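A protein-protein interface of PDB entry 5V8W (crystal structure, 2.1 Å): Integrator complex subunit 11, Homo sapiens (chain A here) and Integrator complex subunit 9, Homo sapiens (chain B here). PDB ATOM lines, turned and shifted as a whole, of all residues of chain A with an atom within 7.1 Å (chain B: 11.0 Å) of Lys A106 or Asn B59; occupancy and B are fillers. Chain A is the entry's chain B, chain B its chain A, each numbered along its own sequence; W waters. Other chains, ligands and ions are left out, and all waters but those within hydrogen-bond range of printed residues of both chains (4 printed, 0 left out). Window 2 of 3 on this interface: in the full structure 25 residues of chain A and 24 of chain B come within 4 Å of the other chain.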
ATOM      1  N   CYS A  27      29.342   1.530   7.380  1.00  0.00           N
ATOM      2  CA  CYS A  27      28.001   1.866   6.944  1.00  0.00           C
ATOM      3  C   CYS A  27      27.626   1.053   5.696  1.00  0.00           C
ATOM      4  O   CYS A  27      28.407   1.019   4.726  1.00  0.00           O
ATOM      5  CB  CYS A  27      27.948   3.355   6.669  1.00  0.00           C
ATOM      6  SG  CYS A  27      26.340   3.879   6.080  1.00  0.00           S
ATOM      7  N   ARG A  28      26.485   0.365   5.727  1.00  0.00           N
ATOM      8  CA  ARG A  28      25.977  -0.425   4.564  1.00  0.00           C
ATOM      9  C   ARG A  28      25.239   0.486   3.577  1.00  0.00           C
ATOM     10  O   ARG A  28      24.085   0.793   3.769  1.00  0.00           O
ATOM     11  CB  ARG A  28      25.033  -1.556   5.020  1.00  0.00           C
ATOM     12  CG  ARG A  28      25.519  -2.363   6.224  1.00  0.00           C
ATOM     13  CD  ARG A  28      24.641  -3.582   6.459  1.00  0.00           C
ATOM     14  NE  ARG A  28      24.920  -4.260   7.735  1.00  0.00           N
ATOM     15  CZ  ARG A  28      24.338  -3.918   8.880  1.00  0.00           C
ATOM     16  NH1 ARG A  28      23.454  -2.912   8.897  1.00  0.00           N
ATOM     17  NH2 ARG A  28      24.619  -4.577  10.009  1.00  0.00           N
ATOM     18  N   VAL A  29      25.930   0.991   2.567  1.00  0.00           N
ATOM     19  CA  VAL A  29      25.296   1.881   1.620  1.00  0.00           C
ATOM     20  C   VAL A  29      24.635   1.043   0.508  1.00  0.00           C
ATOM     21  O   VAL A  29      25.268   0.172  -0.075  1.00  0.00           O
ATOM     22  CB  VAL A  29      26.327   2.868   1.011  1.00  0.00           C
ATOM     23  CG1 VAL A  29      25.682   3.664  -0.136  1.00  0.00           C
ATOM     24  CG2 VAL A  29      26.890   3.809   2.109  1.00  0.00           C
ATOM     25  N   HIS A  30      23.373   1.300   0.221  1.00  0.00           N
ATOM     26  CA  HIS A  30      22.675   0.594  -0.854  1.00  0.00           C
ATOM     27  C   HIS A  30      22.652   1.422  -2.144  1.00  0.00           C
ATOM     28  O   HIS A  30      22.251   2.602  -2.135  1.00  0.00           O
ATOM     29  CB  HIS A  30      21.222   0.288  -0.471  1.00  0.00           C
ATOM     30  CG  HIS A  30      21.072  -0.672   0.662  1.00  0.00           C
ATOM     31  ND1 HIS A  30      22.144  -1.285   1.271  1.00  0.00           N
ATOM     32  CD2 HIS A  30      19.968  -1.124   1.303  1.00  0.00           C
ATOM     33  CE1 HIS A  30      21.708  -2.071   2.241  1.00  0.00           C
ATOM     34  NE2 HIS A  30      20.392  -1.997   2.277  1.00  0.00           N
ATOM     35  N   LEU A  31      23.040   0.800  -3.246  1.00  0.00           N
ATOM     36  CA  LEU A  31      22.988   1.457  -4.540  1.00  0.00           C
ATOM     37  C   LEU A  31      22.242   0.581  -5.528  1.00  0.00           C
ATOM     38  O   LEU A  31      22.416  -0.628  -5.541  1.00  0.00           O
ATOM     39  CB  LEU A  31      24.392   1.748  -5.054  1.00  0.00           C
ATOM     40  CG  LEU A  31      25.111   2.870  -4.333  1.00  0.00           C
ATOM     41  CD1 LEU A  31      26.596   2.849  -4.677  1.00  0.00           C
ATOM     42  CD2 LEU A  31      24.467   4.204  -4.738  1.00  0.00           C
ATOM     43  N   TRP A  90      35.385   3.447   8.180  1.00  0.00           N
ATOM     44  CA  TRP A  90      36.405   4.415   8.598  1.00  0.00           C
ATOM     45  C   TRP A  90      36.523   4.394  10.108  1.00  0.00           C
ATOM     46  O   TRP A  90      35.610   3.926  10.795  1.00  0.00           O
ATOM     47  CB  TRP A  90      36.071   5.840   8.125  1.00  0.00           C
ATOM     48  CG  TRP A  90      34.821   6.471   8.763  1.00  0.00           C
ATOM     49  CD1 TRP A  90      34.807   7.377   9.765  1.00  0.00           C
ATOM     50  CD2 TRP A  90      33.437   6.234   8.417  1.00  0.00           C
ATOM     51  NE1 TRP A  90      33.525   7.738  10.056  1.00  0.00           N
ATOM     52  CE2 TRP A  90      32.662   7.058   9.244  1.00  0.00           C
ATOM     53  CE3 TRP A  90      32.793   5.439   7.465  1.00  0.00           C
ATOM     54  CZ2 TRP A  90      31.248   7.101   9.168  1.00  0.00           C
ATOM     55  CZ3 TRP A  90      31.384   5.473   7.387  1.00  0.00           C
ATOM     56  CH2 TRP A  90      30.633   6.300   8.231  1.00  0.00           C
ATOM     57  N   SER A  99      31.509  10.481   7.144  1.00  0.00           N
ATOM     58  CA  SER A  99      30.117  10.898   7.114  1.00  0.00           C
ATOM     59  C   SER A  99      29.819  11.634   5.817  1.00  0.00           C
ATOM     60  O   SER A  99      28.752  11.463   5.241  1.00  0.00           O
ATOM     61  CB  SER A  99      29.780  11.796   8.294  1.00  0.00           C
ATOM     62  OG  SER A  99      30.644  12.899   8.331  1.00  0.00           O
ATOM     63  N   PHE A 100      30.756  12.458   5.362  1.00  0.00           N
ATOM     64  CA  PHE A 100      30.614  13.102   4.060  1.00  0.00           C
ATOM     65  C   PHE A 100      30.347  12.089   2.912  1.00  0.00           C
ATOM     66  O   PHE A 100      29.505  12.310   2.041  1.00  0.00           O
ATOM     67  CB  PHE A 100      31.855  13.902   3.722  1.00  0.00           C
ATOM     68  CG  PHE A 100      31.777  14.599   2.388  1.00  0.00           C
ATOM     69  CD1 PHE A 100      31.221  15.871   2.293  1.00  0.00           C
ATOM     70  CD2 PHE A 100      32.278  13.994   1.241  1.00  0.00           C
ATOM     71  CE1 PHE A 100      31.145  16.516   1.087  1.00  0.00           C
ATOM     72  CE2 PHE A 100      32.211  14.625   0.027  1.00  0.00           C
ATOM     73  CZ  PHE A 100      31.627  15.892  -0.054  1.00  0.00           C
ATOM     74  N   LEU A 101      31.082  10.989   2.904  1.00  0.00           N
ATOM     75  CA  LEU A 101      30.982  10.040   1.816  1.00  0.00           C
ATOM     76  C   LEU A 101      29.668   9.282   1.884  1.00  0.00           C
ATOM     77  O   LEU A 101      29.052   9.046   0.853  1.00  0.00           O
ATOM     78  CB  LEU A 101      32.171   9.062   1.833  1.00  0.00           C
ATOM     79  CG  LEU A 101      33.478   9.697   1.366  1.00  0.00           C
ATOM     80  CD1 LEU A 101      34.673   8.767   1.595  1.00  0.00           C
ATOM     81  CD2 LEU A 101      33.412  10.118  -0.124  1.00  0.00           C
ATOM     82  N   THR A 102      29.213   8.917   3.082  1.00  0.00           N
ATOM     83  CA  THR A 102      27.964   8.176   3.161  1.00  0.00           C
ATOM     84  C   THR A 102      26.819   9.121   2.843  1.00  0.00           C
ATOM     85  O   THR A 102      25.837   8.735   2.215  1.00  0.00           O
ATOM     86  CB  THR A 102      27.732   7.521   4.532  1.00  0.00           C
ATOM     87  OG1 THR A 102      27.812   8.505   5.578  1.00  0.00           O
ATOM     88  CG2 THR A 102      28.791   6.404   4.759  1.00  0.00           C
ATOM     89  N   SER A 103      26.948  10.366   3.260  1.00  0.00           N
ATOM     90  CA  SER A 103      25.932  11.342   2.885  1.00  0.00           C
ATOM     91  C   SER A 103      25.915  11.513   1.344  1.00  0.00           C
ATOM     92  O   SER A 103      24.842  11.578   0.722  1.00  0.00           O
ATOM     93  CB  SER A 103      26.172  12.685   3.595  1.00  0.00           C
ATOM     94  OG  SER A 103      25.361  13.703   3.029  1.00  0.00           O
ATOM     95  N   LEU A 104      27.098  11.562   0.729  1.00  0.00           N
ATOM     96  CA  LEU A 104      27.182  11.821  -0.722  1.00  0.00           C
ATOM     97  C   LEU A 104      26.487  10.695  -1.487  1.00  0.00           C
ATOM     98  O   LEU A 104      25.674  10.926  -2.399  1.00  0.00           O
ATOM     99  CB  LEU A 104      28.635  11.939  -1.171  1.00  0.00           C
ATOM    100  CG  LEU A 104      28.883  12.206  -2.655  1.00  0.00           C
ATOM    101  CD1 LEU A 104      28.152  13.517  -3.118  1.00  0.00           C
ATOM    102  CD2 LEU A 104      30.398  12.310  -2.886  1.00  0.00           C
ATOM    103  N   LEU A 105      26.776   9.465  -1.081  1.00  0.00           N
ATOM    104  CA  LEU A 105      26.278   8.322  -1.824  1.00  0.00           C
ATOM    105  C   LEU A 105      24.771   8.147  -1.661  1.00  0.00           C
ATOM    106  O   LEU A 105      24.167   7.410  -2.440  1.00  0.00           O
ATOM    107  CB  LEU A 105      27.039   7.045  -1.415  1.00  0.00           C
ATOM    108  CG  LEU A 105      28.515   7.148  -1.793  1.00  0.00           C
ATOM    109  CD1 LEU A 105      29.361   5.999  -1.242  1.00  0.00           C
ATOM    110  CD2 LEU A 105      28.613   7.207  -3.319  1.00  0.00           C
ATOM    111  N   LYS A 106      24.152   8.848  -0.704  1.00  0.00           N
ATOM    112  CA  LYS A 106      22.687   8.826  -0.599  1.00  0.00           C
ATOM    113  C   LYS A 106      22.038   9.379  -1.847  1.00  0.00           C
ATOM    114  O   LYS A 106      20.904   9.035  -2.143  1.00  0.00           O
ATOM    115  CB  LYS A 106      22.168   9.649   0.578  1.00  0.00           C
ATOM    116  CG  LYS A 106      22.411   9.103   1.934  1.00  0.00           C
ATOM    117  CD  LYS A 106      21.752  10.014   2.970  1.00  0.00           C
ATOM    118  CE  LYS A 106      20.289   9.682   3.119  1.00  0.00           C
ATOM    119  NZ  LYS A 106      20.166   8.270   3.604  1.00  0.00           N
ATOM    120  N   LYS A 107      22.730  10.277  -2.552  1.00  0.00           N
ATOM    121  CA  LYS A 107      22.188  10.871  -3.788  1.00  0.00           C
ATOM    122  C   LYS A 107      22.479  10.033  -5.012  1.00  0.00           C
ATOM    123  O   LYS A 107      22.230  10.462  -6.127  1.00  0.00           O
ATOM    124  CB  LYS A 107      22.751  12.268  -4.033  1.00  0.00           C
ATOM    125  CG  LYS A 107      22.319  13.266  -3.003  1.00  0.00           C
ATOM    126  CD  LYS A 107      23.260  13.198  -1.810  1.00  0.00           C
ATOM    127  CE  LYS A 107      22.847  14.157  -0.715  1.00  0.00           C
ATOM    128  NZ  LYS A 107      23.758  14.061   0.469  1.00  0.00           N
ATOM    129  N   GLY A 108      23.040   8.845  -4.811  1.00  0.00           N
ATOM    130  CA  GLY A 108      23.324   7.979  -5.938  1.00  0.00           C
ATOM    131  C   GLY A 108      24.584   8.310  -6.721  1.00  0.00           C
ATOM    132  O   GLY A 108      25.585   8.756  -6.172  1.00  0.00           O
ATOM    133  N   LEU A 109      24.531   8.060  -8.021  1.00  0.00           N
ATOM    134  CA  LEU A 109      25.695   8.176  -8.884  1.00  0.00           C
ATOM    135  C   LEU A 109      25.278   8.905 -10.138  1.00  0.00           C
ATOM    136  O   LEU A 109      24.096   8.955 -10.437  1.00  0.00           O
ATOM    137  CB  LEU A 109      26.248   6.796  -9.229  1.00  0.00           C
ATOM    138  CG  LEU A 109      26.773   5.961  -8.060  1.00  0.00           C
ATOM    139  CD1 LEU A 109      27.168   4.597  -8.605  1.00  0.00           C
ATOM    140  CD2 LEU A 109      27.965   6.664  -7.418  1.00  0.00           C
ATOM    141  N   GLN B  40      17.399  -2.747  16.489  1.00  0.00           N
ATOM    142  CA  GLN B  40      16.611  -2.874  15.268  1.00  0.00           C
ATOM    143  C   GLN B  40      16.872  -1.684  14.338  1.00  0.00           C
ATOM    144  O   GLN B  40      16.872  -1.846  13.116  1.00  0.00           O
ATOM    145  CB  GLN B  40      15.114  -2.984  15.585  1.00  0.00           C
ATOM    146  CG  GLN B  40      14.755  -4.269  16.259  1.00  0.00           C
ATOM    147  CD  GLN B  40      15.092  -5.490  15.399  1.00  0.00           C
ATOM    148  OE1 GLN B  40      15.049  -5.435  14.166  1.00  0.00           O
ATOM    149  NE2 GLN B  40      15.422  -6.599  16.053  1.00  0.00           N
ATOM    150  N   GLU B  41      17.097  -0.506  14.923  1.00  0.00           N
ATOM    151  CA  GLU B  41      17.316   0.734  14.158  1.00  0.00           C
ATOM    152  C   GLU B  41      18.522   0.589  13.270  1.00  0.00           C
ATOM    153  O   GLU B  41      19.644   0.390  13.759  1.00  0.00           O
ATOM    154  CB  GLU B  41      17.531   1.962  15.073  1.00  0.00           C
ATOM    155  CG  GLU B  41      16.311   2.434  15.879  1.00  0.00           C
ATOM    156  CD  GLU B  41      16.119   1.658  17.202  1.00  0.00           C
ATOM    157  OE1 GLU B  41      16.759   0.595  17.395  1.00  0.00           O
ATOM    158  OE2 GLU B  41      15.316   2.110  18.047  1.00  0.00           O
ATOM    159  N   ALA B  42      18.281   0.719  11.973  1.00  0.00           N
ATOM    160  CA  ALA B  42      19.285   0.588  10.938  1.00  0.00           C
ATOM    161  C   ALA B  42      20.049  -0.752  11.033  1.00  0.00           C
ATOM    162  O   ALA B  42      21.196  -0.833  10.617  1.00  0.00           O
ATOM    163  CB  ALA B  42      20.250   1.771  11.003  1.00  0.00           C
ATOM    164  N   GLU B  43      19.399  -1.784  11.578  1.00  0.00           N
ATOM    165  CA  GLU B  43      19.986  -3.121  11.711  1.00  0.00           C
ATOM    166  C   GLU B  43      21.410  -2.999  12.214  1.00  0.00           C
ATOM    167  O   GLU B  43      22.345  -3.435  11.550  1.00  0.00           O
ATOM    168  CB  GLU B  43      19.953  -3.897  10.377  1.00  0.00           C
ATOM    169  CG  GLU B  43      18.568  -3.976   9.742  1.00  0.00           C
ATOM    170  CD  GLU B  43      18.551  -4.756   8.422  1.00  0.00           C
ATOM    171  OE1 GLU B  43      19.462  -4.600   7.580  1.00  0.00           O
ATOM    172  OE2 GLU B  43      17.599  -5.510   8.222  1.00  0.00           O
ATOM    173  N   THR B  44      21.543  -2.394  13.393  1.00  0.00           N
ATOM    174  CA  THR B  44      22.819  -1.974  13.931  1.00  0.00           C
ATOM    175  C   THR B  44      23.431  -3.006  14.838  1.00  0.00           C
ATOM    176  O   THR B  44      22.739  -3.538  15.713  1.00  0.00           O
ATOM    177  CB  THR B  44      22.655  -0.662  14.721  1.00  0.00           C
ATOM    178  OG1 THR B  44      22.264   0.373  13.815  1.00  0.00           O
ATOM    179  CG2 THR B  44      23.943  -0.269  15.396  1.00  0.00           C
ATOM    180  N   LEU B  45      24.721  -3.274  14.632  1.00  0.00           N
ATOM    181  CA  LEU B  45      25.538  -4.023  15.586  1.00  0.00           C
ATOM    182  C   LEU B  45      26.576  -3.048  16.163  1.00  0.00           C
ATOM    183  O   LEU B  45      27.197  -2.271  15.432  1.00  0.00           O
ATOM    184  CB  LEU B  45      26.295  -5.202  14.956  1.00  0.00           C
ATOM    185  CG  LEU B  45      25.728  -6.105  13.880  1.00  0.00           C
ATOM    186  CD1 LEU B  45      26.584  -7.375  13.784  1.00  0.00           C
ATOM    187  CD2 LEU B  45      24.286  -6.398  14.116  1.00  0.00           C
ATOM    188  N   ILE B  55      30.895   0.148  15.165  1.00  0.00           N
ATOM    189  CA  ILE B  55      29.489   0.365  14.881  1.00  0.00           C
ATOM    190  C   ILE B  55      29.228   0.034  13.410  1.00  0.00           C
ATOM    191  O   ILE B  55      29.816   0.663  12.501  1.00  0.00           O
ATOM    192  CB  ILE B  55      29.074   1.818  15.192  1.00  0.00           C
ATOM    193  CG1 ILE B  55      29.181   2.093  16.715  1.00  0.00           C
ATOM    194  CG2 ILE B  55      27.679   2.118  14.629  1.00  0.00           C
ATOM    195  CD1 ILE B  55      28.998   3.593  17.118  1.00  0.00           C
ATOM    196  N   ILE B  56      28.360  -0.953  13.195  1.00  0.00           N
ATOM    197  CA  ILE B  56      27.981  -1.397  11.852  1.00  0.00           C
ATOM    198  C   ILE B  56      26.482  -1.130  11.708  1.00  0.00           C
ATOM    199  O   ILE B  56      25.688  -1.695  12.464  1.00  0.00           O
ATOM    200  CB  ILE B  56      28.292  -2.900  11.639  1.00  0.00           C
ATOM    201  CG1 ILE B  56      29.788  -3.186  11.875  1.00  0.00           C
ATOM    202  CG2 ILE B  56      27.922  -3.365  10.223  1.00  0.00           C
ATOM    203  CD1 ILE B  56      30.022  -4.280  12.849  1.00  0.00           C
ATOM    204  N   CYS B  57      26.100  -0.257  10.773  1.00  0.00           N
ATOM    205  CA  CYS B  57      24.698   0.058  10.570  1.00  0.00           C
ATOM    206  C   CYS B  57      24.369   0.445   9.135  1.00  0.00           C
ATOM    207  O   CYS B  57      25.273   0.748   8.315  1.00  0.00           O
ATOM    208  CB  CYS B  57      24.282   1.202  11.508  1.00  0.00           C
ATOM    209  SG  CYS B  57      25.248   2.726  11.121  1.00  0.00           S
ATOM    210  N   ASP B  58      23.070   0.457   8.838  1.00  0.00           N
ATOM    211  CA  ASP B  58      22.580   0.912   7.535  1.00  0.00           C
ATOM    212  C   ASP B  58      22.854   2.421   7.457  1.00  0.00           C
ATOM    213  O   ASP B  58      23.260   3.035   8.454  1.00  0.00           O
ATOM    214  CB  ASP B  58      21.089   0.573   7.360  1.00  0.00           C
ATOM    215  CG  ASP B  58      20.870  -0.929   7.150  1.00  0.00           C
ATOM    216  OD1 ASP B  58      21.851  -1.625   6.785  1.00  0.00           O
ATOM    217  OD2 ASP B  58      19.738  -1.415   7.325  1.00  0.00           O
ATOM    218  N   ASN B  59      22.653   3.006   6.290  1.00  0.00           N
ATOM    219  CA  ASN B  59      23.001   4.417   6.070  1.00  0.00           C
ATOM    220  C   ASN B  59      21.957   5.381   6.691  1.00  0.00           C
ATOM    221  O   ASN B  59      21.189   6.043   6.002  1.00  0.00           O
ATOM    222  CB  ASN B  59      23.187   4.697   4.553  1.00  0.00           C
ATOM    223  CG  ASN B  59      23.879   6.037   4.302  1.00  0.00           C
ATOM    224  OD1 ASN B  59      24.250   6.714   5.247  1.00  0.00           O
ATOM    225  ND2 ASN B  59      24.061   6.408   3.051  1.00  0.00           N
ATOM    226  N   ASP B  60      21.936   5.425   8.012  1.00  0.00           N
ATOM    227  CA  ASP B  60      21.014   6.254   8.755  1.00  0.00           C
ATOM    228  C   ASP B  60      21.909   7.195   9.553  1.00  0.00           C
ATOM    229  O   ASP B  60      22.354   6.857  10.652  1.00  0.00           O
ATOM    230  CB  ASP B  60      20.112   5.392   9.657  1.00  0.00           C
ATOM    231  CG  ASP B  60      19.069   6.212  10.438  1.00  0.00           C
ATOM    232  OD1 ASP B  60      19.280   7.418  10.680  1.00  0.00           O
ATOM    233  OD2 ASP B  60      18.025   5.630  10.822  1.00  0.00           O
ATOM    234  N   GLU B  61      22.202   8.361   8.991  1.00  0.00           N
ATOM    235  CA  GLU B  61      23.246   9.203   9.551  1.00  0.00           C
ATOM    236  C   GLU B  61      22.878   9.755  10.935  1.00  0.00           C
ATOM    237  O   GLU B  61      23.749   9.926  11.798  1.00  0.00           O
ATOM    238  CB  GLU B  61      23.585  10.357   8.593  1.00  0.00           C
ATOM    239  CG  GLU B  61      24.640  11.338   9.160  1.00  0.00           C
ATOM    240  CD  GLU B  61      26.016  10.677   9.376  1.00  0.00           C
ATOM    241  OE1 GLU B  61      26.156   9.443   9.197  1.00  0.00           O
ATOM    242  OE2 GLU B  61      26.976  11.401   9.714  1.00  0.00           O
ATOM    243  N   MET B  62      21.590  10.010  11.153  1.00  0.00           N
ATOM    244  CA  MET B  62      21.149  10.532  12.442  1.00  0.00           C
ATOM    245  C   MET B  62      21.268   9.483  13.543  1.00  0.00           C
ATOM    246  O   MET B  62      21.649   9.811  14.667  1.00  0.00           O
ATOM    247  CB  MET B  62      19.708  11.075  12.340  1.00  0.00           C
ATOM    248  CG  MET B  62      19.666  12.292  11.378  1.00  0.00           C
ATOM    249  SD  MET B  62      18.256  13.340  11.644  1.00  0.00           S
ATOM    250  CE  MET B  62      16.949  12.287  11.015  1.00  0.00           C
ATOM    251  N   LEU B  63      20.935   8.234  13.213  1.00  0.00           N
ATOM    252  CA  LEU B  63      21.171   7.102  14.113  1.00  0.00           C
ATOM    253  C   LEU B  63      22.676   6.929  14.404  1.00  0.00           C
ATOM    254  O   LEU B  63      23.082   6.808  15.563  1.00  0.00           O
ATOM    255  CB  LEU B  63      20.568   5.829  13.504  1.00  0.00           C
ATOM    256  CG  LEU B  63      20.698   4.476  14.196  1.00  0.00           C
ATOM    257  CD1 LEU B  63      22.040   3.787  13.925  1.00  0.00           C
ATOM    258  CD2 LEU B  63      20.448   4.672  15.697  1.00  0.00           C
ATOM    259  N   ARG B  64      23.496   6.914  13.355  1.00  0.00           N
ATOM    260  CA  ARG B  64      24.943   6.704  13.525  1.00  0.00           C
ATOM    261  C   ARG B  64      25.530   7.801  14.436  1.00  0.00           C
ATOM    262  O   ARG B  64      26.292   7.517  15.327  1.00  0.00           O
ATOM    263  CB  ARG B  64      25.677   6.716  12.165  1.00  0.00           C
ATOM    264  CG  ARG B  64      27.127   6.160  12.244  1.00  0.00           C
ATOM    265  CD  ARG B  64      27.914   6.452  10.970  1.00  0.00           C
ATOM    266  NE  ARG B  64      28.060   7.897  10.795  1.00  0.00           N
ATOM    267  CZ  ARG B  64      29.012   8.628  11.375  1.00  0.00           C
ATOM    268  NH1 ARG B  64      29.939   8.047  12.167  1.00  0.00           N
ATOM    269  NH2 ARG B  64      29.047   9.933  11.151  1.00  0.00           N
ATOM    270  N   VAL B  65      25.111   9.049  14.225  1.00  0.00           N
ATOM    271  CA  VAL B  65      25.636  10.172  14.999  1.00  0.00           C
ATOM    272  C   VAL B  65      25.247  10.003  16.463  1.00  0.00           C
ATOM    273  O   VAL B  65      26.060  10.232  17.381  1.00  0.00           O
ATOM    274  CB  VAL B  65      25.133  11.508  14.420  1.00  0.00           C
ATOM    275  CG1 VAL B  65      25.163  12.612  15.444  1.00  0.00           C
ATOM    276  CG2 VAL B  65      25.934  11.863  13.129  1.00  0.00           C
ATOM    277  N   LEU B  67      24.696   7.194  18.130  1.00  0.00           N
ATOM    278  CA  LEU B  67      25.518   6.149  18.734  1.00  0.00           C
ATOM    279  C   LEU B  67      26.954   6.627  18.902  1.00  0.00           C
ATOM    280  O   LEU B  67      27.570   6.388  19.933  1.00  0.00           O
ATOM    281  CB  LEU B  67      25.487   4.879  17.889  1.00  0.00           C
ATOM    282  CG  LEU B  67      24.071   4.346  17.681  1.00  0.00           C
ATOM    283  CD1 LEU B  67      24.102   3.105  16.805  1.00  0.00           C
ATOM    284  CD2 LEU B  67      23.375   4.059  19.035  1.00  0.00           C
HETATM  285  O   HOH W   1      26.155   7.354   7.557  1.00  0.00           O
HETATM  286  O   HOH W   2      21.554   1.450   4.040  1.00  0.00           O
HETATM  287  O   HOH W   3      24.301   9.586   5.149  1.00  0.00           O
HETATM  288  O   HOH W   4      26.617  10.717   6.568  1.00  0.00           O
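O of Glu B43 lies within hydrogen-bond range of NH1 of Arg A28 (2.9 Å).
O of Asn B59 lies within hydrogen-bond range of NZ of Lys A106 (3.4 Å).
The backbone carbonyl oxygen (O) of Thr A102 lies within hydrogen-bond range of the side-chain amide nitrogen (ND2) of Asn B59 (3.0 Å).
The backbone carbonyl oxygen of Cys B57 sits at hydrogen-bond distance from the backbone NH of Arg A28 (2.9 Å).
The side-chain amide oxygen (OD1) of Asn B59 lies close to the side-chain sulfur (SG) of Cys A27 (3.6 Å).
The side-chain carboxylate of Asp B58 lies within salt-bridge range of the guanidinium group of Arg A28 (2.9 Å).
NH2 of Arg B64 is in salt-bridge range of OE2 of Glu B61, at 2.9 Å.
The backbone NH (N) of Asp B58 lies within hydrogen-bond range of the backbone carbonyl oxygen (O) of Ala B42, 2.9 Å away.
O of Leu B45 sits at hydrogen-bond distance from N of Ile B56 (2.8 Å).
The side-chain hydroxyl (OG1) of Thr A102 sits at hydrogen-bond distance from the backbone carbonyl oxygen (O) of Ser A99, 3.1 Å away.
Among the printed residues, pairs that only touch across the chains: Ser A99 with Glu B61 (3.2 Å), Cys A27 with Cys B57 (3.3 Å), Trp A90 with Arg B64 (3.4 Å), Ser A99 with Arg B64 (3.5 Å), Arg A28 with Ala B42 (3.5 Å), Arg A28 with Ile B56 (3.5 Å), Arg A28 with Asn B59 (3.6 Å), Val A29 with Asn B59 (3.96 Å) and Cys A27 with Asp B58 (3.98 Å).
Lys A106 touches just one residue of chain B: Asn B59.
Of chain B, only Asn B59 comes within 4 Å of Val A29.
No residue of chain B comes within 4 Å of Ser A103.
No residue of chain B comes within 4 Å of Leu A105.
Lys A107 touches none of the printed residues of chain B.
Of the printed residues of chain A, Cys B57 touches Cys A27 (3.3 Å) and Arg A28 (2.9 Å).
Of the printed residues of chain A, Glu B43 touches Arg A28 (2.9 Å).
Of the printed residues of chain A, Ile B56 touches Arg A28.
The nearest residue of chain B that does not touch Lys A106 is Asp B60 (5.5 Å).
The nearest residue of chain A that does not touch Asn B59 is Ser A103 (4.9 Å).
The nearest printed residue of chain B that does not touch Arg A28 is Leu B45 (4.3 Å).
Printed residues of chain B that touch a printed residue of chain A: Ala B42, Glu B43, Ile B56, Cys B57, Asp B58, Asn B59, Glu B61 and Arg B64.
Of the 17 printed residues of chain A, 7 touch a printed residue of chain B.
Printed residues of chain A that touch a printed residue of chain B: Cys A27, Arg A28, Val A29, Trp A90, Ser A99, Thr A102 and Lys A106.
Along chain A the printed residues that touch a printed residue of chain B span positions 27 to 106.
Among the printed residues, Asp or Glu carboxylates within 4 Å of a Lys or Arg side-chain nitrogen of the other chain: Arg A28 with Asp B58.
Water W4 lies within hydrogen-bond range of O of Ser A99 (2.6 Å), OG1 of Thr A102 (2.7 Å), OE1 of Glu B61 (3.0 Å) and N of Ser A103 (3.3 Å).
Water W2 bridges O of Arg A28 and N of Asn B59.
Water W1 lies within hydrogen-bond range of OE1 of Glu B61 (2.7 Å), OG1 of Thr A102 (2.8 Å), OD1 of Asn B59 (3.1 Å) and SG of Cys A27 (3.8 Å).
Water W3 lies within hydrogen-bond range of the side-chain amide oxygen of Asn B59 (2.9 Å), the backbone NH of Ser A103 (3.3 Å) and the backbone carbonyl oxygen of Thr A102 (3.4 Å).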
